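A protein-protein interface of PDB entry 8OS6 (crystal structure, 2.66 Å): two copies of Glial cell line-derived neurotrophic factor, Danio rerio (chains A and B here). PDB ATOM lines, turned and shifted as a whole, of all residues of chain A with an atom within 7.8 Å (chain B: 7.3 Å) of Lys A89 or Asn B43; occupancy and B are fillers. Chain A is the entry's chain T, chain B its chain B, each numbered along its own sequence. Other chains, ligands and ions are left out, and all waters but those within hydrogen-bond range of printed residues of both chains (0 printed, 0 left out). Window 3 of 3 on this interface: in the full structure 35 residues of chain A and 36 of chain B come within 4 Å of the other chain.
No position is printed for both chains.
Of the 13 pairs that touch across the chains among the printed residues, none has its exchanged pair printed and touching as well.
Of the 9 printed residues of chain B, 5 touch a printed residue of chain A.
Along chain B the printed residues that touch a printed residue of chain A span positions 42 to 48.
Hydrophobic or aromatic side chains of chain A that line the printed part of chain B: Leu A18, Phe A30, Phe A72, Leu A88 and His A91.
Among the printed residues, no Asp or Glu carboxylate lies within 4 Å of a Lys or Arg side-chain nitrogen of the other chain.
Among the printed residues, merely in contact across the chains: Lys A90 with Asn B43 (3.3 Å), Phe A30 with Ile B47 (3.4 Å), Phe A72 with Tyr B44 (3.5 Å), Phe A72 with Thr B42 (3.5 Å), His A91 with Tyr B44 (3.5 Å), Leu A18 with Ile B47 (3.7 Å), Phe A30 with Leu B48 (3.8 Å), His A91 with Ile B47 (3.8 Å), Leu A88 with Asn B43 (3.9 Å), Lys A90 with Thr B42 (3.9 Å) and Phe A30 with Tyr B44 (3.99 Å).
OD2 of Asp A75 lies within salt-bridge range of NZ of Lys A89.
O of Ile A76 is in hydrogen-bond range of N of Leu A88 (2.8 Å).
Of chain B, only Asn B43 (2.9 Å) comes within 4 Å of Lys A89.
Of chain A, only Leu A88 (3.9 Å), Lys A89 (2.9 Å) and Lys A90 (3.3 Å) come within 4 Å of Asn B43.
Printed residues of chain B within 4 Å of Leu A18: Ile B47.
Of the printed residues of chain B, His A91 touches Tyr B44 (3.5 Å) and Ile B47 (3.8 Å).
Printed residues of chain B within 4 Å of Phe A72: Thr B42 and Tyr B44.
Glu B41 touches none of the printed residues of chain A.
Ser A77 touches none of the printed residues of chain B.
The nearest residue of chain A that does not touch Asn B43 is His A91 (4.2 Å).
The nearest printed residue of chain B that does not touch His A91 is Asn B43 (4.2 Å).
The backbone carbonyl oxygen (O) of Lys A89 sits at hydrogen-bond distance from the side-chain amide nitrogen (ND2) of Asn B43.
O of Lys A90 sits at hydrogen-bond distance from N of Tyr B44, 2.9 Å away.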
ATOM      1  N   LEU A  18      -0.739  13.238  10.828  1.00  0.00           N
ATOM      2  CA  LEU A  18       0.112  12.060  10.720  1.00  0.00           C
ATOM      3  C   LEU A  18      -0.450  10.878  11.498  1.00  0.00           C
ATOM      4  O   LEU A  18      -0.127   9.729  11.181  1.00  0.00           O
ATOM      5  CB  LEU A  18       1.522  12.384  11.213  1.00  0.00           C
ATOM      6  CG  LEU A  18       2.178  13.631  10.613  1.00  0.00           C
ATOM      7  CD1 LEU A  18       3.681  13.620  10.872  1.00  0.00           C
ATOM      8  CD2 LEU A  18       1.883  13.753   9.124  1.00  0.00           C
ATOM      9  N   LEU A  20      -0.008   9.755  14.678  1.00  0.00           N
ATOM     10  CA  LEU A  20       0.995   9.022  15.437  1.00  0.00           C
ATOM     11  C   LEU A  20       0.695   8.992  16.931  1.00  0.00           C
ATOM     12  O   LEU A  20       1.501   8.457  17.700  1.00  0.00           O
ATOM     13  CB  LEU A  20       2.380   9.636  15.209  1.00  0.00           C
ATOM     14  CG  LEU A  20       2.701  10.044  13.771  1.00  0.00           C
ATOM     15  CD1 LEU A  20       4.114  10.606  13.674  1.00  0.00           C
ATOM     16  CD2 LEU A  20       2.519   8.871  12.824  1.00  0.00           C
ATOM     17  N   TYR A  22      -0.220  11.933  18.794  1.00  0.00           N
ATOM     18  CA  TYR A  22       0.089  13.203  19.434  1.00  0.00           C
ATOM     19  C   TYR A  22      -1.143  14.098  19.503  1.00  0.00           C
ATOM     20  O   TYR A  22      -2.021  14.052  18.637  1.00  0.00           O
ATOM     21  CB  TYR A  22       1.204  13.933  18.681  1.00  0.00           C
ATOM     22  CG  TYR A  22       2.534  13.221  18.699  1.00  0.00           C
ATOM     23  CD1 TYR A  22       3.289  13.155  19.861  1.00  0.00           C
ATOM     24  CD2 TYR A  22       3.039  12.622  17.554  1.00  0.00           C
ATOM     25  CE1 TYR A  22       4.508  12.506  19.885  1.00  0.00           C
ATOM     26  CE2 TYR A  22       4.259  11.971  17.568  1.00  0.00           C
ATOM     27  CZ  TYR A  22       4.989  11.917  18.736  1.00  0.00           C
ATOM     28  OH  TYR A  22       6.205  11.270  18.760  1.00  0.00           O
ATOM     29  N   PHE A  30       6.095  17.482   5.069  1.00  0.00           N
ATOM     30  CA  PHE A  30       6.468  16.084   4.906  1.00  0.00           C
ATOM     31  C   PHE A  30       6.874  15.838   3.460  1.00  0.00           C
ATOM     32  O   PHE A  30       6.153  16.218   2.533  1.00  0.00           O
ATOM     33  CB  PHE A  30       5.301  15.179   5.309  1.00  0.00           C
ATOM     34  CG  PHE A  30       5.512  13.726   5.002  1.00  0.00           C
ATOM     35  CD1 PHE A  30       6.235  12.918   5.862  1.00  0.00           C
ATOM     36  CD2 PHE A  30       4.967  13.163   3.861  1.00  0.00           C
ATOM     37  CE1 PHE A  30       6.422  11.579   5.583  1.00  0.00           C
ATOM     38  CE2 PHE A  30       5.149  11.825   3.578  1.00  0.00           C
ATOM     39  CZ  PHE A  30       5.877  11.032   4.439  1.00  0.00           C
ATOM     40  N   PHE A  72      17.455  10.888   4.913  1.00  0.00           N
ATOM     41  CA  PHE A  72      16.323  11.381   5.681  1.00  0.00           C
ATOM     42  C   PHE A  72      16.508  12.853   6.039  1.00  0.00           C
ATOM     43  O   PHE A  72      17.622  13.383   6.064  1.00  0.00           O
ATOM     44  CB  PHE A  72      16.125  10.546   6.947  1.00  0.00           C
ATOM     45  CG  PHE A  72      15.363   9.273   6.718  1.00  0.00           C
ATOM     46  CD1 PHE A  72      14.036   9.311   6.320  1.00  0.00           C
ATOM     47  CD2 PHE A  72      15.965   8.041   6.907  1.00  0.00           C
ATOM     48  CE1 PHE A  72      13.328   8.147   6.107  1.00  0.00           C
ATOM     49  CE2 PHE A  72      15.260   6.870   6.697  1.00  0.00           C
ATOM     50  CZ  PHE A  72      13.940   6.924   6.296  1.00  0.00           C
ATOM     51  N   ASP A  73      15.387  13.511   6.317  1.00  0.00           N
ATOM     52  CA  ASP A  73      15.382  14.932   6.618  1.00  0.00           C
ATOM     53  C   ASP A  73      15.797  15.180   8.065  1.00  0.00           C
ATOM     54  O   ASP A  73      15.804  14.273   8.903  1.00  0.00           O
ATOM     55  CB  ASP A  73      13.991  15.517   6.362  1.00  0.00           C
ATOM     56  CG  ASP A  73      14.018  17.013   6.104  1.00  0.00           C
ATOM     57  OD1 ASP A  73      14.933  17.695   6.612  1.00  0.00           O
ATOM     58  OD2 ASP A  73      13.117  17.504   5.389  1.00  0.00           O
ATOM     59  N   ASP A  74      16.146  16.432   8.350  1.00  0.00           N
ATOM     60  CA  ASP A  74      16.478  16.833   9.708  1.00  0.00           C
ATOM     61  C   ASP A  74      15.332  16.496  10.659  1.00  0.00           C
ATOM     62  O   ASP A  74      14.172  16.357  10.257  1.00  0.00           O
ATOM     63  CB  ASP A  74      16.773  18.333   9.770  1.00  0.00           C
ATOM     64  CG  ASP A  74      18.003  18.723   8.975  1.00  0.00           C
ATOM     65  OD1 ASP A  74      19.059  18.080   9.150  1.00  0.00           O
ATOM     66  OD2 ASP A  74      17.914  19.673   8.171  1.00  0.00           O
ATOM     67  N   ASP A  75      15.669  16.370  11.938  1.00  0.00           N
ATOM     68  CA  ASP A  75      14.661  16.084  12.948  1.00  0.00           C
ATOM     69  C   ASP A  75      13.739  17.284  13.135  1.00  0.00           C
ATOM     70  O   ASP A  75      14.110  18.430  12.871  1.00  0.00           O
ATOM     71  CB  ASP A  75      15.323  15.723  14.278  1.00  0.00           C
ATOM     72  CG  ASP A  75      16.231  14.514  14.170  1.00  0.00           C
ATOM     73  OD1 ASP A  75      15.898  13.581  13.409  1.00  0.00           O
ATOM     74  OD2 ASP A  75      17.282  14.500  14.847  1.00  0.00           O
ATOM     75  N   ILE A  76      12.521  17.007  13.594  1.00  0.00           N
ATOM     76  CA  ILE A  76      11.534  18.039  13.876  1.00  0.00           C
ATOM     77  C   ILE A  76      11.038  17.845  15.301  1.00  0.00           C
ATOM     78  O   ILE A  76      10.979  16.724  15.812  1.00  0.00           O
ATOM     79  CB  ILE A  76      10.358  18.000  12.876  1.00  0.00           C
ATOM     80  CG1 ILE A  76       9.584  19.320  12.910  1.00  0.00           C
ATOM     81  CG2 ILE A  76       9.421  16.850  13.199  1.00  0.00           C
ATOM     82  CD1 ILE A  76       8.578  19.473  11.785  1.00  0.00           C
ATOM     83  N   SER A  77      10.688  18.955  15.946  1.00  0.00           N
ATOM     84  CA  SER A  77      10.178  18.942  17.308  1.00  0.00           C
ATOM     85  C   SER A  77       8.966  19.859  17.390  1.00  0.00           C
ATOM     86  O   SER A  77       8.800  20.771  16.575  1.00  0.00           O
ATOM     87  CB  SER A  77      11.251  19.383  18.312  1.00  0.00           C
ATOM     88  OG  SER A  77      12.352  18.489  18.303  1.00  0.00           O
ATOM     89  N   THR A  87       9.893  15.041  20.059  1.00  0.00           N
ATOM     90  CA  THR A  87      10.815  15.110  18.935  1.00  0.00           C
ATOM     91  C   THR A  87      10.645  13.877  18.058  1.00  0.00           C
ATOM     92  O   THR A  87      10.543  12.755  18.562  1.00  0.00           O
ATOM     93  CB  THR A  87      12.276  15.212  19.408  1.00  0.00           C
ATOM     94  OG1 THR A  87      12.787  13.903  19.693  1.00  0.00           O
ATOM     95  CG2 THR A  87      12.377  16.073  20.662  1.00  0.00           C
ATOM     96  N   LEU A  88      10.610  14.094  16.746  1.00  0.00           N
ATOM     97  CA  LEU A  88      10.504  13.020  15.769  1.00  0.00           C
ATOM     98  C   LEU A  88      11.780  12.943  14.944  1.00  0.00           C
ATOM     99  O   LEU A  88      12.398  13.969  14.640  1.00  0.00           O
ATOM    100  CB  LEU A  88       9.305  13.226  14.840  1.00  0.00           C
ATOM    101  CG  LEU A  88       7.931  12.848  15.391  1.00  0.00           C
ATOM    102  CD1 LEU A  88       6.893  12.899  14.278  1.00  0.00           C
ATOM    103  CD2 LEU A  88       7.942  11.474  16.035  1.00  0.00           C
ATOM    104  N   LYS A  89      12.162  11.721  14.578  1.00  0.00           N
ATOM    105  CA  LYS A  89      13.370  11.461  13.811  1.00  0.00           C
ATOM    106  C   LYS A  89      13.033  10.568  12.626  1.00  0.00           C
ATOM    107  O   LYS A  89      12.148   9.712  12.708  1.00  0.00           O
ATOM    108  CB  LYS A  89      14.441  10.797  14.679  1.00  0.00           C
ATOM    109  CG  LYS A  89      14.846  11.614  15.892  1.00  0.00           C
ATOM    110  CD  LYS A  89      15.597  10.760  16.898  1.00  0.00           C
ATOM    111  CE  LYS A  89      16.495  11.605  17.785  1.00  0.00           C
ATOM    112  NZ  LYS A  89      17.627  12.201  17.018  1.00  0.00           N
ATOM    113  N   LYS A  90      13.750  10.776  11.524  1.00  0.00           N
ATOM    114  CA  LYS A  90      13.558  10.011  10.294  1.00  0.00           C
ATOM    115  C   LYS A  90      12.075   9.931   9.927  1.00  0.00           C
ATOM    116  O   LYS A  90      11.471   8.859   9.861  1.00  0.00           O
ATOM    117  CB  LYS A  90      14.171   8.614  10.422  1.00  0.00           C
ATOM    118  CG  LYS A  90      15.685   8.625  10.553  1.00  0.00           C
ATOM    119  CD  LYS A  90      16.259   7.223  10.640  1.00  0.00           C
ATOM    120  CE  LYS A  90      17.763   7.266  10.850  1.00  0.00           C
ATOM    121  NZ  LYS A  90      18.391   5.921  10.722  1.00  0.00           N
ATOM    122  N   HIS A  91      11.498  11.108   9.684  1.00  0.00           N
ATOM    123  CA  HIS A  91      10.095  11.243   9.324  1.00  0.00           C
ATOM    124  C   HIS A  91       9.881  11.756   7.910  1.00  0.00           C
ATOM    125  O   HIS A  91       8.884  11.398   7.282  1.00  0.00           O
ATOM    126  CB  HIS A  91       9.395  12.201  10.294  1.00  0.00           C
ATOM    127  CG  HIS A  91       9.933  13.596  10.243  1.00  0.00           C
ATOM    128  ND1 HIS A  91      11.076  13.975  10.911  1.00  0.00           N
ATOM    129  CD2 HIS A  91       9.497  14.697   9.587  1.00  0.00           C
ATOM    130  CE1 HIS A  91      11.317  15.253  10.676  1.00  0.00           C
ATOM    131  NE2 HIS A  91      10.372  15.714   9.877  1.00  0.00           N
ATOM    132  N   SER A  92      10.787  12.587   7.400  1.00  0.00           N
ATOM    133  CA  SER A  92      10.665  13.194   6.085  1.00  0.00           C
ATOM    134  C   SER A  92      11.878  12.830   5.238  1.00  0.00           C
ATOM    135  O   SER A  92      12.990  12.671   5.751  1.00  0.00           O
ATOM    136  CB  SER A  92      10.532  14.721   6.200  1.00  0.00           C
ATOM    137  OG  SER A  92      10.424  15.337   4.929  1.00  0.00           O
ATOM    138  N   GLU B  41      11.463  -0.657   9.878  1.00  0.00           N
ATOM    139  CA  GLU B  41      10.710   0.485   9.381  1.00  0.00           C
ATOM    140  C   GLU B  41      10.869   1.682  10.311  1.00  0.00           C
ATOM    141  O   GLU B  41      11.002   1.541  11.531  1.00  0.00           O
ATOM    142  CB  GLU B  41       9.230   0.133   9.228  1.00  0.00           C
ATOM    143  CG  GLU B  41       8.934  -0.782   8.048  1.00  0.00           C
ATOM    144  CD  GLU B  41       7.464  -0.793   7.667  1.00  0.00           C
ATOM    145  OE1 GLU B  41       6.671  -0.085   8.324  1.00  0.00           O
ATOM    146  OE2 GLU B  41       7.104  -1.506   6.707  1.00  0.00           O
ATOM    147  N   THR B  42      10.850   2.869   9.716  1.00  0.00           N
ATOM    148  CA  THR B  42      11.071   4.128  10.410  1.00  0.00           C
ATOM    149  C   THR B  42       9.756   4.891  10.541  1.00  0.00           C
ATOM    150  O   THR B  42       8.706   4.459  10.058  1.00  0.00           O
ATOM    151  CB  THR B  42      12.108   4.969   9.663  1.00  0.00           C
ATOM    152  OG1 THR B  42      11.746   5.052   8.278  1.00  0.00           O
ATOM    153  CG2 THR B  42      13.494   4.355   9.787  1.00  0.00           C
ATOM    154  N   ASN B  43       9.826   6.046  11.213  1.00  0.00           N
ATOM    155  CA  ASN B  43       8.672   6.939  11.278  1.00  0.00           C
ATOM    156  C   ASN B  43       8.150   7.256   9.883  1.00  0.00           C
ATOM    157  O   ASN B  43       6.935   7.272   9.652  1.00  0.00           O
ATOM    158  CB  ASN B  43       9.049   8.231  12.007  1.00  0.00           C
ATOM    159  CG  ASN B  43       8.938   8.108  13.515  1.00  0.00           C
ATOM    160  OD1 ASN B  43       7.993   7.515  14.035  1.00  0.00           O
ATOM    161  ND2 ASN B  43       9.904   8.677  14.227  1.00  0.00           N
ATOM    162  N   TYR B  44       9.060   7.517   8.941  1.00  0.00           N
ATOM    163  CA  TYR B  44       8.671   7.782   7.559  1.00  0.00           C
ATOM    164  C   TYR B  44       7.709   6.719   7.042  1.00  0.00           C
ATOM    165  O   TYR B  44       6.690   7.035   6.418  1.00  0.00           O
ATOM    166  CB  TYR B  44       9.922   7.852   6.681  1.00  0.00           C
ATOM    167  CG  TYR B  44       9.643   7.962   5.200  1.00  0.00           C
ATOM    168  CD1 TYR B  44       9.519   6.827   4.413  1.00  0.00           C
ATOM    169  CD2 TYR B  44       9.517   9.199   4.587  1.00  0.00           C
ATOM    170  CE1 TYR B  44       9.269   6.923   3.061  1.00  0.00           C
ATOM    171  CE2 TYR B  44       9.266   9.303   3.235  1.00  0.00           C
ATOM    172  CZ  TYR B  44       9.142   8.163   2.477  1.00  0.00           C
ATOM    173  OH  TYR B  44       8.892   8.263   1.129  1.00  0.00           O
ATOM    174  N   ASP B  45       8.020   5.446   7.290  1.00  0.00           N
ATOM    175  CA  ASP B  45       7.131   4.379   6.844  1.00  0.00           C
ATOM    176  C   ASP B  45       5.788   4.441   7.564  1.00  0.00           C
ATOM    177  O   ASP B  45       4.736   4.250   6.940  1.00  0.00           O
ATOM    178  CB  ASP B  45       7.794   3.017   7.060  1.00  0.00           C
ATOM    179  CG  ASP B  45       9.041   2.831   6.213  1.00  0.00           C
ATOM    180  OD1 ASP B  45       9.456   3.797   5.539  1.00  0.00           O
ATOM    181  OD2 ASP B  45       9.606   1.716   6.219  1.00  0.00           O
ATOM    182  N   LYS B  46       5.799   4.713   8.873  1.00  0.00           N
ATOM    183  CA  LYS B  46       4.550   4.727   9.628  1.00  0.00           C
ATOM    184  C   LYS B  46       3.658   5.885   9.196  1.00  0.00           C
ATOM    185  O   LYS B  46       2.429   5.752   9.165  1.00  0.00           O
ATOM    186  CB  LYS B  46       4.838   4.804  11.128  1.00  0.00           C
ATOM    187  CG  LYS B  46       5.869   3.794  11.622  1.00  0.00           C
ATOM    188  CD  LYS B  46       5.591   2.387  11.098  1.00  0.00           C
ATOM    189  CE  LYS B  46       6.616   1.381  11.613  1.00  0.00           C
ATOM    190  NZ  LYS B  46       6.366   0.010  11.085  1.00  0.00           N
ATOM    191  N   ILE B  47       4.259   7.028   8.865  1.00  0.00           N
ATOM    192  CA  ILE B  47       3.482   8.149   8.342  1.00  0.00           C
ATOM    193  C   ILE B  47       2.820   7.763   7.025  1.00  0.00           C
ATOM    194  O   ILE B  47       1.641   8.060   6.796  1.00  0.00           O
ATOM    195  CB  ILE B  47       4.381   9.389   8.184  1.00  0.00           C
ATOM    196  CG1 ILE B  47       4.671  10.010   9.552  1.00  0.00           C
ATOM    197  CG2 ILE B  47       3.735  10.404   7.253  1.00  0.00           C
ATOM    198  CD1 ILE B  47       5.855  10.953   9.559  1.00  0.00           C
ATOM    199  N   LEU B  48       3.569   7.095   6.143  1.00  0.00           N
ATOM    200  CA  LEU B  48       3.021   6.716   4.843  1.00  0.00           C
ATOM    201  C   LEU B  48       1.823   5.789   5.000  1.00  0.00           C
ATOM    202  O   LEU B  48       0.797   5.965   4.331  1.00  0.00           O
ATOM    203  CB  LEU B  48       4.104   6.049   3.994  1.00  0.00           C
ATOM    204  CG  LEU B  48       5.173   6.965   3.398  1.00  0.00           C
ATOM    205  CD1 LEU B  48       6.165   6.152   2.580  1.00  0.00           C
ATOM    206  CD2 LEU B  48       4.545   8.056   2.545  1.00  0.00           C
ATOM    207  N   ASN B  49       1.935   4.791   5.878  1.00  0.00           N
ATOM    208  CA  ASN B  49       0.825   3.869   6.086  1.00  0.00           C
ATOM    209  C   ASN B  49      -0.374   4.579   6.703  1.00  0.00           C
ATOM    210  O   ASN B  49      -1.522   4.303   6.336  1.00  0.00           O
ATOM    211  CB  ASN B  49       1.276   2.704   6.968  1.00  0.00           C
ATOM    212  CG  ASN B  49       0.165   1.706   7.232  1.00  0.00           C
ATOM    213  OD1 ASN B  49      -0.902   1.770   6.622  1.00  0.00           O
ATOM    214  ND2 ASN B  49       0.414   0.773   8.143  1.00  0.00           N
